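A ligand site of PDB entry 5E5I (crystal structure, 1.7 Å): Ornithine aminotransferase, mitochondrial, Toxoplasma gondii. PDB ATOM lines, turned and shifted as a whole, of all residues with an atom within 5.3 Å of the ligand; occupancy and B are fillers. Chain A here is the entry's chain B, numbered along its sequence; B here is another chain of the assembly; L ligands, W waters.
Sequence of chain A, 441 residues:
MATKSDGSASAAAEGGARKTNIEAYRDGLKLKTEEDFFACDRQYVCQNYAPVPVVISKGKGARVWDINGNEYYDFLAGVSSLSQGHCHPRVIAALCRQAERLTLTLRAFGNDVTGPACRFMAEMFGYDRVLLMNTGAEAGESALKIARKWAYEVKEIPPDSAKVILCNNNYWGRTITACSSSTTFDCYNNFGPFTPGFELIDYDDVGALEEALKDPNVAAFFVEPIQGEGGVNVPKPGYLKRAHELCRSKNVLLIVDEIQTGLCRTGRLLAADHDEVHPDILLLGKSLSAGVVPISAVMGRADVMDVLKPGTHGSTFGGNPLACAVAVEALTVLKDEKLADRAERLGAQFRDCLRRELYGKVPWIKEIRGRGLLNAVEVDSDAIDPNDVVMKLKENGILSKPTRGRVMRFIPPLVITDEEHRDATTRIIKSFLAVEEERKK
The side-chain amino group of Lys 286 lies within hydrogen-bond range of an oxygen (O3) of the ligand (2.7 Å). The side-chain hydroxyl (OG1) of Thr 316 of chain B is in hydrogen-bond range of an oxygen (O6) of the ligand (2.6 Å). OD2 of Asp 257 is in hydrogen-bond range of N2 of the ligand (2.7 Å). NE2 of Gln 260 lies within hydrogen-bond range of O3 of the ligand (2.9 Å). The backbone NH (N) of Ser 315 of chain B lies within hydrogen-bond range of an oxygen (O1) of the ligand, 3.0 Å away. The backbone NH of Thr 316 of chain B sits at hydrogen-bond distance from an oxygen (O6) of the ligand (2.9 Å). An oxygen (O5) of the ligand is in hydrogen-bond range of the backbone NH of Gly 136, at 2.8 Å. An oxygen (O7) of the ligand is in hydrogen-bond range of the backbone NH (N) of Ala 137, 2.8 Å away. The side-chain hydroxyl (OH) of Tyr 49 lies within hydrogen-bond range of an oxygen (O2) of the ligand.
N of Ser 315 of chain B sits at hydrogen-bond distance from OH of Tyr 49 (3.0 Å). NE of Arg 174 sits at hydrogen-bond distance from OH of Tyr 171, 3.0 Å away. NE2 of Gln 260 lies within hydrogen-bond range of OE2 of Glu 229, 3.3 Å away. The side-chain hydroxyl (OG1) of Thr 135 is in hydrogen-bond range of the backbone NH (N) of Glu 138 of chain A, 3.1 Å away. The backbone NH (N) of Tyr 171 is in hydrogen-bond range of the side-chain carboxylate (OE2) of Glu 224 (3.2 Å). The backbone NH (N) of Ile 259 lies within hydrogen-bond range of the side-chain carboxylate (OD1) of Asp 257 (2.9 Å). The side-chain carboxylate (OE2) of Glu 138 of chain B sits at hydrogen-bond distance from the side-chain hydroxyl (OG1) of Thr 135 (2.9 Å).
Val 79 touches the ligand. Thr 135 touches the ligand (CB to O7, 3.9 Å). Tyr 171 touches the ligand (CE1 to N1, 3.5 Å). Trp 172 touches the ligand. Glu 224 touches the ligand (OE1 to C10, 3.6 Å). Glu 229 touches the ligand. Ile 259 touches the ligand. Gly 314 of chain B touches the ligand. Hydrophobic or aromatic side chains within 4 Å of the ligand: Tyr 49, Val 79, Ala 137, Tyr 171 and Ile 259. The nearest printed residue that does not touch the ligand is Gly 173 (4.1 Å).
Water W11 bridges an oxygen (O7) of the ligand (2.8 Å) and the backbone NH of Arg 174 (3.1 Å). Water W4 lies within hydrogen-bond range of O5 of the ligand (2.8 Å), N of Phe 317 of chain B (2.9 Å) and OG of Ser 315 of chain B (3.4 Å). Water W7 lies within hydrogen-bond range of the side-chain hydroxyl of Tyr 171 (2.6 Å) and an oxygen (O6) of the ligand (2.8 Å). Water W3 lies within hydrogen-bond range of O5 of the ligand (2.9 Å), N of Lys 286 (3.0 Å) and N of Gly 136 (3.4 Å). Water W8 lies within hydrogen-bond range of the guanidinium group (NH2) of Arg 174 (2.8 Å), an oxygen (O1) of the ligand (3.0 Å) and the side-chain hydroxyl (OH) of Tyr 171 (3.2 Å). Water W9 lies within hydrogen-bond range of N of Arg 107 of chain B, O of Ser 315 of chain B, O2 of the ligand, OH of Tyr 49 and O of Thr 316 of chain B.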
ATOM      1  N   TYR A  49     -18.394 -19.536  -5.735  1.00  0.00           N
ATOM      2  CA  TYR A  49     -18.073 -20.713  -6.534  1.00  0.00           C
ATOM      3  C   TYR A  49     -18.583 -21.964  -5.887  1.00  0.00           C
ATOM      4  O   TYR A  49     -18.596 -22.041  -4.673  1.00  0.00           O
ATOM      5  CB  TYR A  49     -16.579 -20.826  -6.800  1.00  0.00           C
ATOM      6  CG  TYR A  49     -16.116 -19.947  -7.928  1.00  0.00           C
ATOM      7  CD1 TYR A  49     -15.893 -18.568  -7.738  1.00  0.00           C
ATOM      8  CD2 TYR A  49     -15.904 -20.488  -9.191  1.00  0.00           C
ATOM      9  CE1 TYR A  49     -15.488 -17.770  -8.815  1.00  0.00           C
ATOM     10  CE2 TYR A  49     -15.461 -19.692 -10.240  1.00  0.00           C
ATOM     11  CZ  TYR A  49     -15.256 -18.354 -10.042  1.00  0.00           C
ATOM     12  OH  TYR A  49     -14.846 -17.620 -11.117  1.00  0.00           O
ATOM     13  N   GLY A  78      -7.580 -23.551 -16.910  1.00  0.00           N
ATOM     14  CA  GLY A  78      -7.976 -22.172 -16.733  1.00  0.00           C
ATOM     15  C   GLY A  78      -8.982 -21.735 -17.763  1.00  0.00           C
ATOM     16  O   GLY A  78      -9.120 -20.549 -18.009  1.00  0.00           O
ATOM     17  N   VAL A  79      -9.711 -22.699 -18.289  1.00  0.00           N
ATOM     18  CA  VAL A  79     -10.621 -22.536 -19.426  1.00  0.00           C
ATOM     19  C   VAL A  79      -9.801 -21.914 -20.589  1.00  0.00           C
ATOM     20  O   VAL A  79     -10.098 -20.859 -21.110  1.00  0.00           O
ATOM     21  CB  VAL A  79     -11.883 -21.725 -19.158  1.00  0.00           C
ATOM     22  CG1 VAL A  79     -12.842 -22.062 -20.264  1.00  0.00           C
ATOM     23  CG2 VAL A  79     -12.524 -22.113 -17.830  1.00  0.00           C
ATOM     24  N   THR A 135      -8.278  -7.884 -17.691  1.00  0.00           N
ATOM     25  CA  THR A 135      -9.083  -9.059 -17.708  1.00  0.00           C
ATOM     26  C   THR A 135      -9.897  -9.143 -19.014  1.00  0.00           C
ATOM     27  O   THR A 135     -10.033  -8.182 -19.776  1.00  0.00           O
ATOM     28  CB  THR A 135     -10.094  -9.035 -16.535  1.00  0.00           C
ATOM     29  OG1 THR A 135     -11.035  -7.996 -16.696  1.00  0.00           O
ATOM     30  CG2 THR A 135      -9.396  -8.846 -15.204  1.00  0.00           C
ATOM     31  N   GLY A 136     -10.513 -10.285 -19.176  1.00  0.00           N
ATOM     32  CA  GLY A 136     -11.332 -10.537 -20.348  1.00  0.00           C
ATOM     33  C   GLY A 136     -12.514  -9.598 -20.341  1.00  0.00           C
ATOM     34  O   GLY A 136     -12.847  -8.965 -21.371  1.00  0.00           O
ATOM     35  N   ALA A 137     -13.123  -9.501 -19.171  1.00  0.00           N
ATOM     36  CA  ALA A 137     -14.268  -8.598 -19.034  1.00  0.00           C
ATOM     37  C   ALA A 137     -13.893  -7.161 -19.436  1.00  0.00           C
ATOM     38  O   ALA A 137     -14.685  -6.474 -20.050  1.00  0.00           O
ATOM     39  CB  ALA A 137     -14.770  -8.643 -17.573  1.00  0.00           C
ATOM     40  N   GLU A 138     -12.734  -6.663 -18.957  1.00  0.00           N
ATOM     41  CA  GLU A 138     -12.266  -5.322 -19.308  1.00  0.00           C
ATOM     42  C   GLU A 138     -12.036  -5.145 -20.857  1.00  0.00           C
ATOM     43  O   GLU A 138     -12.262  -4.029 -21.395  1.00  0.00           O
ATOM     44  CB  GLU A 138     -10.996  -4.953 -18.547  1.00  0.00           C
ATOM     45  CG  GLU A 138     -11.219  -4.615 -17.099  1.00  0.00           C
ATOM     46  CD  GLU A 138      -9.961  -4.169 -16.374  1.00  0.00           C
ATOM     47  OE1 GLU A 138      -8.828  -4.488 -16.862  1.00  0.00           O
ATOM     48  OE2 GLU A 138     -10.154  -3.405 -15.367  1.00  0.00           O
ATOM     49  N   TYR A 171     -20.838 -15.385 -23.390  1.00  0.00           N
ATOM     50  CA  TYR A 171     -20.193 -15.053 -22.123  1.00  0.00           C
ATOM     51  C   TYR A 171     -19.003 -14.155 -22.421  1.00  0.00           C
ATOM     52  O   TYR A 171     -18.196 -14.484 -23.261  1.00  0.00           O
ATOM     53  CB  TYR A 171     -19.690 -16.278 -21.343  1.00  0.00           C
ATOM     54  CG  TYR A 171     -19.175 -15.953 -19.939  1.00  0.00           C
ATOM     55  CD1 TYR A 171     -17.867 -15.514 -19.744  1.00  0.00           C
ATOM     56  CD2 TYR A 171     -19.993 -16.108 -18.826  1.00  0.00           C
ATOM     57  CE1 TYR A 171     -17.395 -15.203 -18.481  1.00  0.00           C
ATOM     58  CE2 TYR A 171     -19.517 -15.804 -17.552  1.00  0.00           C
ATOM     59  CZ  TYR A 171     -18.182 -15.402 -17.391  1.00  0.00           C
ATOM     60  OH  TYR A 171     -17.723 -15.084 -16.172  1.00  0.00           O
ATOM     61  N   TRP A 172     -18.944 -12.983 -21.790  1.00  0.00           N
ATOM     62  CA  TRP A 172     -17.804 -12.116 -21.954  1.00  0.00           C
ATOM     63  C   TRP A 172     -17.312 -11.508 -20.663  1.00  0.00           C
ATOM     64  O   TRP A 172     -16.326 -10.824 -20.712  1.00  0.00           O
ATOM     65  CB  TRP A 172     -17.970 -11.052 -23.010  1.00  0.00           C
ATOM     66  CG  TRP A 172     -19.017 -10.032 -22.794  1.00  0.00           C
ATOM     67  CD1 TRP A 172     -20.310 -10.113 -23.239  1.00  0.00           C
ATOM     68  CD2 TRP A 172     -18.872  -8.751 -22.210  1.00  0.00           C
ATOM     69  NE1 TRP A 172     -20.967  -8.940 -22.988  1.00  0.00           N
ATOM     70  CE2 TRP A 172     -20.116  -8.080 -22.374  1.00  0.00           C
ATOM     71  CE3 TRP A 172     -17.817  -8.069 -21.571  1.00  0.00           C
ATOM     72  CZ2 TRP A 172     -20.316  -6.820 -21.909  1.00  0.00           C
ATOM     73  CZ3 TRP A 172     -18.034  -6.787 -21.121  1.00  0.00           C
ATOM     74  CH2 TRP A 172     -19.300  -6.186 -21.267  1.00  0.00           C
ATOM     75  N   GLY A 173     -17.944 -11.820 -19.540  1.00  0.00           N
ATOM     76  CA  GLY A 173     -17.517 -11.230 -18.251  1.00  0.00           C
ATOM     77  C   GLY A 173     -18.614 -11.106 -17.271  1.00  0.00           C
ATOM     78  O   GLY A 173     -19.742 -11.567 -17.501  1.00  0.00           O
ATOM     79  N   ARG A 174     -18.252 -10.486 -16.149  1.00  0.00           N
ATOM     80  CA  ARG A 174     -19.133 -10.313 -15.015  1.00  0.00           C
ATOM     81  C   ARG A 174     -19.409  -8.866 -14.560  1.00  0.00           C
ATOM     82  O   ARG A 174     -19.832  -8.678 -13.435  1.00  0.00           O
ATOM     83  CB  ARG A 174     -18.559 -11.112 -13.851  1.00  0.00           C
ATOM     84  CG  ARG A 174     -18.487 -12.633 -14.102  1.00  0.00           C
ATOM     85  CD  ARG A 174     -19.882 -13.278 -14.126  1.00  0.00           C
ATOM     86  NE  ARG A 174     -19.793 -14.732 -14.058  1.00  0.00           N
ATOM     87  CZ  ARG A 174     -20.775 -15.532 -13.659  1.00  0.00           C
ATOM     88  NH1 ARG A 174     -21.945 -15.056 -13.171  1.00  0.00           N
ATOM     89  NH2 ARG A 174     -20.537 -16.831 -13.614  1.00  0.00           N
ATOM     90  N   GLU A 224     -18.476 -14.794 -30.465  1.00  0.00           N
ATOM     91  CA  GLU A 224     -17.411 -15.789 -30.229  1.00  0.00           C
ATOM     92  C   GLU A 224     -17.353 -16.739 -31.422  1.00  0.00           C
ATOM     93  O   GLU A 224     -18.392 -17.179 -31.879  1.00  0.00           O
ATOM     94  CB  GLU A 224     -17.770 -16.665 -29.008  1.00  0.00           C
ATOM     95  CG  GLU A 224     -17.823 -15.841 -27.719  1.00  0.00           C
ATOM     96  CD  GLU A 224     -18.475 -16.576 -26.520  1.00  0.00           C
ATOM     97  OE1 GLU A 224     -17.858 -17.439 -25.867  1.00  0.00           O
ATOM     98  OE2 GLU A 224     -19.685 -16.277 -26.261  1.00  0.00           O
ATOM     99  N   GLU A 229     -18.225 -20.649 -22.650  1.00  0.00           N
ATOM    100  CA  GLU A 229     -19.045 -20.938 -21.453  1.00  0.00           C
ATOM    101  C   GLU A 229     -20.440 -21.452 -21.838  1.00  0.00           C
ATOM    102  O   GLU A 229     -21.045 -22.223 -21.087  1.00  0.00           O
ATOM    103  CB  GLU A 229     -19.158 -19.733 -20.501  1.00  0.00           C
ATOM    104  CG  GLU A 229     -17.796 -19.236 -19.918  1.00  0.00           C
ATOM    105  CD  GLU A 229     -17.006 -20.304 -19.236  1.00  0.00           C
ATOM    106  OE1 GLU A 229     -17.269 -20.626 -18.048  1.00  0.00           O
ATOM    107  OE2 GLU A 229     -16.062 -20.815 -19.901  1.00  0.00           O
ATOM    108  N   ASP A 257     -14.551 -12.186 -30.070  1.00  0.00           N
ATOM    109  CA  ASP A 257     -13.990 -12.494 -28.776  1.00  0.00           C
ATOM    110  C   ASP A 257     -13.211 -13.826 -28.877  1.00  0.00           C
ATOM    111  O   ASP A 257     -13.798 -14.891 -28.984  1.00  0.00           O
ATOM    112  CB  ASP A 257     -15.112 -12.587 -27.757  1.00  0.00           C
ATOM    113  CG  ASP A 257     -14.600 -12.807 -26.342  1.00  0.00           C
ATOM    114  OD1 ASP A 257     -13.402 -13.192 -26.173  1.00  0.00           O
ATOM    115  OD2 ASP A 257     -15.383 -12.647 -25.372  1.00  0.00           O
ATOM    116  N   ILE A 259     -10.880 -14.642 -26.591  1.00  0.00           N
ATOM    117  CA  ILE A 259     -10.264 -14.782 -25.249  1.00  0.00           C
ATOM    118  C   ILE A 259     -10.147 -16.255 -24.858  1.00  0.00           C
ATOM    119  O   ILE A 259      -9.114 -16.700 -24.313  1.00  0.00           O
ATOM    120  CB  ILE A 259     -11.062 -13.920 -24.234  1.00  0.00           C
ATOM    121  CG1 ILE A 259     -10.833 -12.434 -24.545  1.00  0.00           C
ATOM    122  CG2 ILE A 259     -10.641 -14.206 -22.816  1.00  0.00           C
ATOM    123  CD1 ILE A 259     -11.880 -11.550 -23.867  1.00  0.00           C
ATOM    124  N   GLN A 260     -11.139 -17.043 -25.226  1.00  0.00           N
ATOM    125  CA  GLN A 260     -11.100 -18.500 -24.944  1.00  0.00           C
ATOM    126  C   GLN A 260     -10.653 -19.313 -26.173  1.00  0.00           C
ATOM    127  O   GLN A 260      -9.865 -20.260 -26.025  1.00  0.00           O
ATOM    128  CB  GLN A 260     -12.444 -19.013 -24.410  1.00  0.00           C
ATOM    129  CG  GLN A 260     -12.410 -20.490 -24.076  1.00  0.00           C
ATOM    130  CD  GLN A 260     -13.666 -21.020 -23.412  1.00  0.00           C
ATOM    131  OE1 GLN A 260     -13.970 -22.204 -23.551  1.00  0.00           O
ATOM    132  NE2 GLN A 260     -14.358 -20.194 -22.640  1.00  0.00           N
ATOM    133  N   LYS A 286      -6.689 -14.517 -21.325  1.00  0.00           N
ATOM    134  CA  LYS A 286      -6.383 -15.863 -20.806  1.00  0.00           C
ATOM    135  C   LYS A 286      -5.000 -16.418 -21.086  1.00  0.00           C
ATOM    136  O   LYS A 286      -4.099 -16.145 -20.307  1.00  0.00           O
ATOM    137  CB  LYS A 286      -7.470 -16.817 -21.242  1.00  0.00           C
ATOM    138  CG  LYS A 286      -8.776 -16.410 -20.556  1.00  0.00           C
ATOM    139  CD  LYS A 286      -9.889 -17.361 -20.864  1.00  0.00           C
ATOM    140  CE  LYS A 286     -11.186 -16.850 -20.311  1.00  0.00           C
ATOM    141  NZ  LYS A 286     -12.158 -17.867 -20.824  1.00  0.00           N
ATOM    142  N   LEU B 106      -8.040 -21.519 -11.208  1.00  0.00           N
ATOM    143  CA  LEU B 106      -9.447 -21.039 -11.330  1.00  0.00           C
ATOM    144  C   LEU B 106     -10.087 -21.412 -10.002  1.00  0.00           C
ATOM    145  O   LEU B 106      -9.626 -22.353  -9.308  1.00  0.00           O
ATOM    146  CB  LEU B 106     -10.243 -21.751 -12.395  1.00  0.00           C
ATOM    147  CG  LEU B 106      -9.874 -21.593 -13.854  1.00  0.00           C
ATOM    148  CD1 LEU B 106     -10.755 -22.546 -14.656  1.00  0.00           C
ATOM    149  CD2 LEU B 106     -10.075 -20.145 -14.333  1.00  0.00           C
ATOM    150  N   ARG B 107     -11.181 -20.736  -9.667  1.00  0.00           N
ATOM    151  CA  ARG B 107     -11.865 -21.045  -8.431  1.00  0.00           C
ATOM    152  C   ARG B 107     -12.746 -22.274  -8.585  1.00  0.00           C
ATOM    153  O   ARG B 107     -13.374 -22.751  -7.621  1.00  0.00           O
ATOM    154  CB  ARG B 107     -12.506 -19.820  -7.862  1.00  0.00           C
ATOM    155  CG  ARG B 107     -11.496 -18.868  -7.228  1.00  0.00           C
ATOM    156  CD  ARG B 107     -12.162 -17.690  -6.581  1.00  0.00           C
ATOM    157  NE  ARG B 107     -13.028 -18.241  -5.531  1.00  0.00           N
ATOM    158  CZ  ARG B 107     -14.051 -17.608  -4.986  1.00  0.00           C
ATOM    159  NH1 ARG B 107     -14.342 -16.353  -5.346  1.00  0.00           N
ATOM    160  NH2 ARG B 107     -14.783 -18.258  -4.080  1.00  0.00           N
ATOM    161  N   GLU B 138     -13.157  -3.683 -11.286  1.00  0.00           N
ATOM    162  CA  GLU B 138     -13.877  -4.914 -11.029  1.00  0.00           C
ATOM    163  C   GLU B 138     -14.340  -4.969  -9.581  1.00  0.00           C
ATOM    164  O   GLU B 138     -15.325  -5.579  -9.309  1.00  0.00           O
ATOM    165  CB  GLU B 138     -13.017  -6.174 -11.329  1.00  0.00           C
ATOM    166  CG  GLU B 138     -12.923  -6.506 -12.783  1.00  0.00           C
ATOM    167  CD  GLU B 138     -12.155  -7.790 -13.070  1.00  0.00           C
ATOM    168  OE1 GLU B 138     -11.350  -8.234 -12.183  1.00  0.00           O
ATOM    169  OE2 GLU B 138     -12.388  -8.324 -14.198  1.00  0.00           O
ATOM    170  N   GLY B 314     -18.100 -14.313 -10.896  1.00  0.00           N
ATOM    171  CA  GLY B 314     -16.836 -15.088 -11.134  1.00  0.00           C
ATOM    172  C   GLY B 314     -15.785 -14.180 -11.776  1.00  0.00           C
ATOM    173  O   GLY B 314     -15.963 -12.977 -11.888  1.00  0.00           O
ATOM    174  N   SER B 315     -14.618 -14.767 -12.058  1.00  0.00           N
ATOM    175  CA  SER B 315     -13.517 -14.038 -12.667  1.00  0.00           C
ATOM    176  C   SER B 315     -12.468 -15.080 -12.932  1.00  0.00           C
ATOM    177  O   SER B 315     -12.218 -15.888 -12.059  1.00  0.00           O
ATOM    178  CB  SER B 315     -12.913 -13.028 -11.697  1.00  0.00           C
ATOM    179  OG  SER B 315     -11.712 -12.494 -12.230  1.00  0.00           O
ATOM    180  N   THR B 316     -11.923 -15.118 -14.127  1.00  0.00           N
ATOM    181  CA  THR B 316     -10.912 -16.123 -14.443  1.00  0.00           C
ATOM    182  C   THR B 316      -9.720 -16.018 -13.499  1.00  0.00           C
ATOM    183  O   THR B 316      -9.350 -16.997 -12.863  1.00  0.00           O
ATOM    184  CB  THR B 316     -10.418 -16.014 -15.886  1.00  0.00           C
ATOM    185  OG1 THR B 316     -11.506 -16.307 -16.815  1.00  0.00           O
ATOM    186  CG2 THR B 316      -9.291 -17.002 -16.168  1.00  0.00           C
ATOM    187  N   PHE B 317      -9.161 -14.846 -13.410  1.00  0.00           N
ATOM    188  CA  PHE B 317      -7.945 -14.687 -12.574  1.00  0.00           C
ATOM    189  C   PHE B 317      -8.173 -14.249 -11.150  1.00  0.00           C
ATOM    190  O   PHE B 317      -7.226 -14.156 -10.388  1.00  0.00           O
ATOM    191  CB  PHE B 317      -6.992 -13.697 -13.248  1.00  0.00           C
ATOM    192  CG  PHE B 317      -6.256 -14.253 -14.425  1.00  0.00           C
ATOM    193  CD1 PHE B 317      -5.024 -14.867 -14.254  1.00  0.00           C
ATOM    194  CD2 PHE B 317      -6.775 -14.124 -15.716  1.00  0.00           C
ATOM    195  CE1 PHE B 317      -4.346 -15.377 -15.351  1.00  0.00           C
ATOM    196  CE2 PHE B 317      -6.102 -14.642 -16.825  1.00  0.00           C
ATOM    197  CZ  PHE B 317      -4.863 -15.269 -16.622  1.00  0.00           C
HETATM  198  O1  LIG L   1     -15.108 -16.962 -14.092  1.00  0.00           O
HETATM  199  C1  LIG L   1     -14.579 -18.099 -14.197  1.00  0.00           C
HETATM  200  O2  LIG L   1     -14.275 -18.924 -13.312  1.00  0.00           O
HETATM  201  C2  LIG L   1     -14.240 -18.625 -15.546  1.00  0.00           C
HETATM  202  C3  LIG L   1     -14.844 -17.818 -16.665  1.00  0.00           C
HETATM  203  C4  LIG L   1     -14.370 -18.067 -18.053  1.00  0.00           C
HETATM  204  C5  LIG L   1     -13.487 -19.038 -18.303  1.00  0.00           C
HETATM  205  N1  LIG L   1     -14.677 -17.275 -19.285  1.00  0.00           N
HETATM  206  C6  LIG L   1     -14.012 -16.139 -19.510  1.00  0.00           C
HETATM  207  C7  LIG L   1     -14.216 -15.317 -20.783  1.00  0.00           C
HETATM  208  C8  LIG L   1     -14.415 -15.966 -22.035  1.00  0.00           C
HETATM  209  O3  LIG L   1     -14.403 -17.306 -22.199  1.00  0.00           O
HETATM  210  C9  LIG L   1     -14.651 -15.211 -23.160  1.00  0.00           C
HETATM  211  C10 LIG L   1     -14.866 -15.882 -24.516  1.00  0.00           C
HETATM  212  N2  LIG L   1     -14.700 -13.876 -23.064  1.00  0.00           N
HETATM  213  C11 LIG L   1     -14.486 -13.236 -21.922  1.00  0.00           C
HETATM  214  C12 LIG L   1     -14.266 -13.926 -20.740  1.00  0.00           C
HETATM  215  C13 LIG L   1     -14.035 -13.172 -19.444  1.00  0.00           C
HETATM  216  O4  LIG L   1     -12.645 -13.124 -19.060  1.00  0.00           O
HETATM  217  P1  LIG L   1     -12.283 -12.826 -17.513  1.00  0.00           P
HETATM  218  O5  LIG L   1     -10.782 -12.676 -17.651  1.00  0.00           O
HETATM  219  O6  LIG L   1     -12.716 -14.000 -16.699  1.00  0.00           O
HETATM  220  O7  LIG L   1     -12.978 -11.523 -17.191  1.00  0.00           O
HETATM  221  O   HOH W   1     -14.459 -21.536 -13.458  1.00  0.00           O
HETATM  222  O   HOH W   2     -12.228 -11.073 -14.467  1.00  0.00           O
HETATM  223  O   HOH W   3      -8.631 -13.135 -19.583  1.00  0.00           O
HETATM  224  O   HOH W   4      -9.731 -12.510 -15.043  1.00  0.00           O
HETATM  225  O   HOH W   5     -17.050 -18.103 -23.128  1.00  0.00           O
HETATM  226  O   HOH W   6     -15.433 -18.386 -26.662  1.00  0.00           O
HETATM  227  O   HOH W   7     -15.261 -14.502 -15.552  1.00  0.00           O
HETATM  228  O   HOH W   8     -17.977 -17.700 -14.414  1.00  0.00           O
HETATM  229  O   HOH W   9     -11.795 -18.668 -11.426  1.00  0.00           O
HETATM  230  O   HOH W  10     -13.243 -16.915 -27.350  1.00  0.00           O
HETATM  231  O   HOH W  11     -15.341 -11.526 -15.660  1.00  0.00           O
